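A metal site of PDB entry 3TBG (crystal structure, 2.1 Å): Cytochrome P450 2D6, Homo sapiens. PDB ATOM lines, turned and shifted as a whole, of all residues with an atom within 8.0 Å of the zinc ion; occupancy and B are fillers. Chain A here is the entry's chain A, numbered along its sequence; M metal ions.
The side-chain carboxylate of Asp 248 sits close to the backbone NH of Gly 170 (3.3 Å).
The side-chain carboxylate (OD1) of Asp 248 sits close to the backbone NH (N) of Thr 250, at 3.5 Å.
The backbone carbonyl oxygen of Cys 169 lies close to a ring nitrogen (NE2) of His 236 (3.5 Å).
The side-chain hydroxyl (OG1) of Thr 239 sits at hydrogen-bond distance from the backbone carbonyl oxygen (O) of His 236 (3.1 Å).
N of Arg 247 is in hydrogen-bond range of OE1 of Glu 251 (2.9 Å).
SG of Cys 169 is in hydrogen-bond range of OG1 of Thr 168 (3.5 Å).
Cys 169 touches the zinc ion.
Of the 22 residues printed, 4 come within 4 Å of the zinc ion.
The nearest printed residue that does not touch the zinc ion is Arg 247 (4.4 Å).
The zinc ion is bound by OE2 of Glu 251 (1.9 Å), NE2 of His 236 (2.0 Å) and OD2 of Asp 248 (2.0 Å).
The zinc ion has three donor atoms within binding distance.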
ATOM      1  N   TRP A 130     -10.403 -23.802 -29.595  1.00  0.00           N
ATOM      2  CA  TRP A 130     -10.567 -25.034 -28.813  1.00  0.00           C
ATOM      3  C   TRP A 130     -11.410 -26.050 -29.596  1.00  0.00           C
ATOM      4  O   TRP A 130     -11.097 -27.250 -29.601  1.00  0.00           O
ATOM      5  CB  TRP A 130     -11.249 -24.739 -27.473  1.00  0.00           C
ATOM      6  CG  TRP A 130     -10.404 -24.003 -26.471  1.00  0.00           C
ATOM      7  CD1 TRP A 130      -9.092 -24.250 -26.159  1.00  0.00           C
ATOM      8  CD2 TRP A 130     -10.834 -22.941 -25.607  1.00  0.00           C
ATOM      9  NE1 TRP A 130      -8.686 -23.416 -25.142  1.00  0.00           N
ATOM     10  CE2 TRP A 130      -9.729 -22.597 -24.792  1.00  0.00           C
ATOM     11  CE3 TRP A 130     -12.042 -22.256 -25.446  1.00  0.00           C
ATOM     12  CZ2 TRP A 130      -9.811 -21.589 -23.821  1.00  0.00           C
ATOM     13  CZ3 TRP A 130     -12.124 -21.248 -24.474  1.00  0.00           C
ATOM     14  CH2 TRP A 130     -11.004 -20.931 -23.669  1.00  0.00           C
ATOM     15  N   ALA A 165     -15.325 -28.291 -21.316  1.00  0.00           N
ATOM     16  CA  ALA A 165     -14.194 -28.281 -20.408  1.00  0.00           C
ATOM     17  C   ALA A 165     -13.284 -27.116 -20.758  1.00  0.00           C
ATOM     18  O   ALA A 165     -12.754 -26.449 -19.869  1.00  0.00           O
ATOM     19  CB  ALA A 165     -13.421 -29.602 -20.505  1.00  0.00           C
ATOM     20  N   SER A 166     -13.085 -26.875 -22.055  1.00  0.00           N
ATOM     21  CA  SER A 166     -12.233 -25.766 -22.503  1.00  0.00           C
ATOM     22  C   SER A 166     -12.857 -24.431 -22.108  1.00  0.00           C
ATOM     23  O   SER A 166     -12.176 -23.543 -21.618  1.00  0.00           O
ATOM     24  CB  SER A 166     -12.040 -25.808 -24.025  1.00  0.00           C
ATOM     25  OG  SER A 166     -11.433 -27.016 -24.417  1.00  0.00           O
ATOM     26  N   LEU A 167     -14.162 -24.305 -22.339  1.00  0.00           N
ATOM     27  CA  LEU A 167     -14.920 -23.095 -22.011  1.00  0.00           C
ATOM     28  C   LEU A 167     -14.921 -22.767 -20.531  1.00  0.00           C
ATOM     29  O   LEU A 167     -14.727 -21.623 -20.136  1.00  0.00           O
ATOM     30  CB  LEU A 167     -16.376 -23.238 -22.476  1.00  0.00           C
ATOM     31  CG  LEU A 167     -17.419 -22.391 -21.718  1.00  0.00           C
ATOM     32  CD1 LEU A 167     -17.261 -20.923 -22.079  1.00  0.00           C
ATOM     33  CD2 LEU A 167     -18.839 -22.861 -22.071  1.00  0.00           C
ATOM     34  N   THR A 168     -15.159 -23.795 -19.702  1.00  0.00           N
ATOM     35  CA  THR A 168     -15.247 -23.619 -18.261  1.00  0.00           C
ATOM     36  C   THR A 168     -13.935 -23.690 -17.488  1.00  0.00           C
ATOM     37  O   THR A 168     -13.717 -22.879 -16.598  1.00  0.00           O
ATOM     38  CB  THR A 168     -16.193 -24.667 -17.649  1.00  0.00           C
ATOM     39  OG1 THR A 168     -15.697 -25.977 -17.933  1.00  0.00           O
ATOM     40  CG2 THR A 168     -17.600 -24.516 -18.200  1.00  0.00           C
ATOM     41  N   CYS A 169     -13.071 -24.651 -17.811  1.00  0.00           N
ATOM     42  CA  CYS A 169     -11.808 -24.832 -17.090  1.00  0.00           C
ATOM     43  C   CYS A 169     -10.550 -24.499 -17.878  1.00  0.00           C
ATOM     44  O   CYS A 169      -9.448 -24.568 -17.344  1.00  0.00           O
ATOM     45  CB  CYS A 169     -11.692 -26.276 -16.595  1.00  0.00           C
ATOM     46  SG  CYS A 169     -13.137 -26.910 -15.737  1.00  0.00           S
ATOM     47  N   GLY A 170     -10.703 -24.147 -19.147  1.00  0.00           N
ATOM     48  CA  GLY A 170      -9.538 -23.820 -19.947  1.00  0.00           C
ATOM     49  C   GLY A 170      -8.621 -25.003 -20.251  1.00  0.00           C
ATOM     50  O   GLY A 170      -7.408 -24.825 -20.402  1.00  0.00           O
ATOM     51  N   ARG A 171      -9.166 -26.210 -20.341  1.00  0.00           N
ATOM     52  CA  ARG A 171      -8.349 -27.396 -20.635  1.00  0.00           C
ATOM     53  C   ARG A 171      -9.204 -28.480 -21.256  1.00  0.00           C
ATOM     54  O   ARG A 171     -10.433 -28.406 -21.239  1.00  0.00           O
ATOM     55  CB  ARG A 171      -7.762 -27.983 -19.361  1.00  0.00           C
ATOM     56  CG  ARG A 171      -8.819 -28.619 -18.461  1.00  0.00           C
ATOM     57  CD  ARG A 171      -8.191 -29.565 -17.447  1.00  0.00           C
ATOM     58  NE  ARG A 171      -7.574 -30.701 -18.118  1.00  0.00           N
ATOM     59  CZ  ARG A 171      -6.887 -31.659 -17.505  1.00  0.00           C
ATOM     60  NH1 ARG A 171      -6.698 -31.612 -16.189  1.00  0.00           N
ATOM     61  NH2 ARG A 171      -6.382 -32.657 -18.226  1.00  0.00           N
ATOM     62  N   HIS A 236      -8.242 -26.279 -10.712  1.00  0.00           N
ATOM     63  CA  HIS A 236      -8.220 -25.093 -11.557  1.00  0.00           C
ATOM     64  C   HIS A 236      -7.953 -23.851 -10.728  1.00  0.00           C
ATOM     65  O   HIS A 236      -7.260 -22.947 -11.163  1.00  0.00           O
ATOM     66  CB  HIS A 236      -9.567 -24.911 -12.272  1.00  0.00           C
ATOM     67  CG  HIS A 236      -9.549 -23.824 -13.313  1.00  0.00           C
ATOM     68  ND1 HIS A 236     -10.695 -23.384 -13.938  1.00  0.00           N
ATOM     69  CD2 HIS A 236      -8.536 -23.110 -13.843  1.00  0.00           C
ATOM     70  CE1 HIS A 236     -10.386 -22.447 -14.813  1.00  0.00           C
ATOM     71  NE2 HIS A 236      -9.087 -22.260 -14.773  1.00  0.00           N
ATOM     72  N   ARG A 237      -8.530 -23.811  -9.533  1.00  0.00           N
ATOM     73  CA  ARG A 237      -8.389 -22.682  -8.620  1.00  0.00           C
ATOM     74  C   ARG A 237      -6.922 -22.507  -8.278  1.00  0.00           C
ATOM     75  O   ARG A 237      -6.448 -21.389  -8.083  1.00  0.00           O
ATOM     76  CB  ARG A 237      -9.218 -22.938  -7.353  1.00  0.00           C
ATOM     77  CG  ARG A 237      -9.106 -21.868  -6.267  1.00  0.00           C
ATOM     78  CD  ARG A 237     -10.437 -21.157  -5.982  1.00  0.00           C
ATOM     79  NE  ARG A 237     -11.563 -22.088  -5.846  1.00  0.00           N
ATOM     80  CZ  ARG A 237     -12.768 -21.755  -5.373  1.00  0.00           C
ATOM     81  NH1 ARG A 237     -13.009 -20.508  -4.972  1.00  0.00           N
ATOM     82  NH2 ARG A 237     -13.735 -22.657  -5.307  1.00  0.00           N
ATOM     83  N   THR A 239      -4.395 -23.325 -10.309  1.00  0.00           N
ATOM     84  CA  THR A 239      -3.630 -22.895 -11.470  1.00  0.00           C
ATOM     85  C   THR A 239      -4.000 -21.511 -12.028  1.00  0.00           C
ATOM     86  O   THR A 239      -3.276 -20.953 -12.839  1.00  0.00           O
ATOM     87  CB  THR A 239      -3.722 -23.934 -12.615  1.00  0.00           C
ATOM     88  OG1 THR A 239      -5.078 -24.082 -13.046  1.00  0.00           O
ATOM     89  CG2 THR A 239      -3.208 -25.288 -12.132  1.00  0.00           C
ATOM     90  N   TRP A 240      -5.121 -20.962 -11.564  1.00  0.00           N
ATOM     91  CA  TRP A 240      -5.582 -19.659 -12.019  1.00  0.00           C
ATOM     92  C   TRP A 240      -4.582 -18.544 -11.722  1.00  0.00           C
ATOM     93  O   TRP A 240      -4.065 -18.443 -10.617  1.00  0.00           O
ATOM     94  CB  TRP A 240      -6.912 -19.318 -11.325  1.00  0.00           C
ATOM     95  CG  TRP A 240      -7.396 -17.909 -11.542  1.00  0.00           C
ATOM     96  CD1 TRP A 240      -7.372 -17.195 -12.709  1.00  0.00           C
ATOM     97  CD2 TRP A 240      -8.092 -17.088 -10.592  1.00  0.00           C
ATOM     98  NE1 TRP A 240      -8.008 -15.990 -12.543  1.00  0.00           N
ATOM     99  CE2 TRP A 240      -8.466 -15.903 -11.257  1.00  0.00           C
ATOM    100  CE3 TRP A 240      -8.440 -17.243  -9.242  1.00  0.00           C
ATOM    101  CZ2 TRP A 240      -9.174 -14.869 -10.613  1.00  0.00           C
ATOM    102  CZ3 TRP A 240      -9.140 -16.216  -8.600  1.00  0.00           C
ATOM    103  CH2 TRP A 240      -9.493 -15.049  -9.291  1.00  0.00           C
ATOM    104  N   ASP A 241      -4.311 -17.723 -12.732  1.00  0.00           N
ATOM    105  CA  ASP A 241      -3.414 -16.587 -12.579  1.00  0.00           C
ATOM    106  C   ASP A 241      -4.289 -15.328 -12.635  1.00  0.00           C
ATOM    107  O   ASP A 241      -4.583 -14.822 -13.706  1.00  0.00           O
ATOM    108  CB  ASP A 241      -2.381 -16.549 -13.712  1.00  0.00           C
ATOM    109  CG  ASP A 241      -1.366 -15.427 -13.536  1.00  0.00           C
ATOM    110  OD1 ASP A 241      -0.401 -15.346 -14.325  1.00  0.00           O
ATOM    111  OD2 ASP A 241      -1.544 -14.622 -12.612  1.00  0.00           O
ATOM    112  N   PRO A 245      -5.794 -11.591 -17.664  1.00  0.00           N
ATOM    113  CA  PRO A 245      -7.238 -11.543 -17.928  1.00  0.00           C
ATOM    114  C   PRO A 245      -7.790 -12.968 -17.874  1.00  0.00           C
ATOM    115  O   PRO A 245      -7.076 -13.925 -18.189  1.00  0.00           O
ATOM    116  CB  PRO A 245      -7.319 -10.965 -19.335  1.00  0.00           C
ATOM    117  CG  PRO A 245      -6.094 -10.075 -19.398  1.00  0.00           C
ATOM    118  CD  PRO A 245      -5.043 -10.946 -18.752  1.00  0.00           C
ATOM    119  N   PRO A 246      -9.058 -13.132 -17.463  1.00  0.00           N
ATOM    120  CA  PRO A 246      -9.678 -14.457 -17.392  1.00  0.00           C
ATOM    121  C   PRO A 246      -9.498 -15.206 -18.702  1.00  0.00           C
ATOM    122  O   PRO A 246      -9.750 -14.660 -19.771  1.00  0.00           O
ATOM    123  CB  PRO A 246     -11.132 -14.128 -17.105  1.00  0.00           C
ATOM    124  CG  PRO A 246     -11.041 -12.907 -16.267  1.00  0.00           C
ATOM    125  CD  PRO A 246      -9.975 -12.093 -16.986  1.00  0.00           C
ATOM    126  N   ARG A 247      -9.064 -16.456 -18.631  1.00  0.00           N
ATOM    127  CA  ARG A 247      -8.829 -17.257 -19.818  1.00  0.00           C
ATOM    128  C   ARG A 247     -10.031 -18.155 -20.155  1.00  0.00           C
ATOM    129  O   ARG A 247     -10.157 -18.646 -21.269  1.00  0.00           O
ATOM    130  CB  ARG A 247      -7.608 -18.144 -19.571  1.00  0.00           C
ATOM    131  CG  ARG A 247      -6.736 -18.343 -20.769  1.00  0.00           C
ATOM    132  CD  ARG A 247      -5.530 -19.170 -20.377  1.00  0.00           C
ATOM    133  NE  ARG A 247      -5.954 -20.479 -19.918  1.00  0.00           N
ATOM    134  CZ  ARG A 247      -6.250 -21.497 -20.721  1.00  0.00           C
ATOM    135  NH1 ARG A 247      -6.145 -21.363 -22.038  1.00  0.00           N
ATOM    136  NH2 ARG A 247      -6.665 -22.636 -20.205  1.00  0.00           N
ATOM    137  N   ASP A 248     -10.891 -18.350 -19.164  1.00  0.00           N
ATOM    138  CA  ASP A 248     -12.064 -19.204 -19.336  1.00  0.00           C
ATOM    139  C   ASP A 248     -13.169 -18.721 -18.402  1.00  0.00           C
ATOM    140  O   ASP A 248     -12.960 -17.819 -17.598  1.00  0.00           O
ATOM    141  CB  ASP A 248     -11.684 -20.648 -19.032  1.00  0.00           C
ATOM    142  CG  ASP A 248     -10.862 -20.769 -17.758  1.00  0.00           C
ATOM    143  OD1 ASP A 248     -11.349 -20.329 -16.699  1.00  0.00           O
ATOM    144  OD2 ASP A 248      -9.735 -21.297 -17.816  1.00  0.00           O
ATOM    145  N   LEU A 249     -14.344 -19.344 -18.512  1.00  0.00           N
ATOM    146  CA  LEU A 249     -15.494 -18.936 -17.729  1.00  0.00           C
ATOM    147  C   LEU A 249     -15.343 -19.061 -16.222  1.00  0.00           C
ATOM    148  O   LEU A 249     -15.826 -18.205 -15.474  1.00  0.00           O
ATOM    149  CB  LEU A 249     -16.755 -19.696 -18.216  1.00  0.00           C
ATOM    150  CG  LEU A 249     -18.080 -19.223 -17.592  1.00  0.00           C
ATOM    151  CD1 LEU A 249     -19.241 -19.487 -18.538  1.00  0.00           C
ATOM    152  CD2 LEU A 249     -18.291 -19.923 -16.270  1.00  0.00           C
ATOM    153  N   THR A 250     -14.659 -20.099 -15.748  1.00  0.00           N
ATOM    154  CA  THR A 250     -14.471 -20.260 -14.306  1.00  0.00           C
ATOM    155  C   THR A 250     -13.569 -19.144 -13.757  1.00  0.00           C
ATOM    156  O   THR A 250     -13.780 -18.665 -12.638  1.00  0.00           O
ATOM    157  CB  THR A 250     -13.879 -21.654 -13.971  1.00  0.00           C
ATOM    158  OG1 THR A 250     -14.839 -22.666 -14.294  1.00  0.00           O
ATOM    159  CG2 THR A 250     -13.547 -21.748 -12.489  1.00  0.00           C
ATOM    160  N   GLU A 251     -12.586 -18.719 -14.535  1.00  0.00           N
ATOM    161  CA  GLU A 251     -11.688 -17.652 -14.062  1.00  0.00           C
ATOM    162  C   GLU A 251     -12.472 -16.334 -14.006  1.00  0.00           C
ATOM    163  O   GLU A 251     -12.276 -15.535 -13.095  1.00  0.00           O
ATOM    164  CB  GLU A 251     -10.460 -17.527 -14.972  1.00  0.00           C
ATOM    165  CG  GLU A 251      -9.480 -18.666 -14.755  1.00  0.00           C
ATOM    166  CD  GLU A 251      -8.264 -18.611 -15.671  1.00  0.00           C
ATOM    167  OE1 GLU A 251      -7.949 -17.529 -16.193  1.00  0.00           O
ATOM    168  OE2 GLU A 251      -7.607 -19.665 -15.832  1.00  0.00           O
ATOM    169  N   ALA A 252     -13.356 -16.115 -14.965  1.00  0.00           N
ATOM    170  CA  ALA A 252     -14.154 -14.901 -14.970  1.00  0.00           C
ATOM    171  C   ALA A 252     -15.078 -14.915 -13.750  1.00  0.00           C
ATOM    172  O   ALA A 252     -15.281 -13.899 -13.115  1.00  0.00           O
ATOM    173  CB  ALA A 252     -14.959 -14.801 -16.261  1.00  0.00           C
ATOM    174  N   LEU A 254     -14.558 -16.565 -10.870  1.00  0.00           N
ATOM    175  CA  LEU A 254     -13.716 -16.407  -9.689  1.00  0.00           C
ATOM    176  C   LEU A 254     -13.354 -14.936  -9.465  1.00  0.00           C
ATOM    177  O   LEU A 254     -13.416 -14.448  -8.348  1.00  0.00           O
ATOM    178  CB  LEU A 254     -12.429 -17.247  -9.821  1.00  0.00           C
ATOM    179  CG  LEU A 254     -12.615 -18.768  -9.808  1.00  0.00           C
ATOM    180  CD1 LEU A 254     -11.264 -19.453 -10.048  1.00  0.00           C
ATOM    181  CD2 LEU A 254     -13.187 -19.205  -8.475  1.00  0.00           C
HETATM  182 ZN    ZN M   1      -8.338 -21.330 -16.351  1.00  0.00          ZN
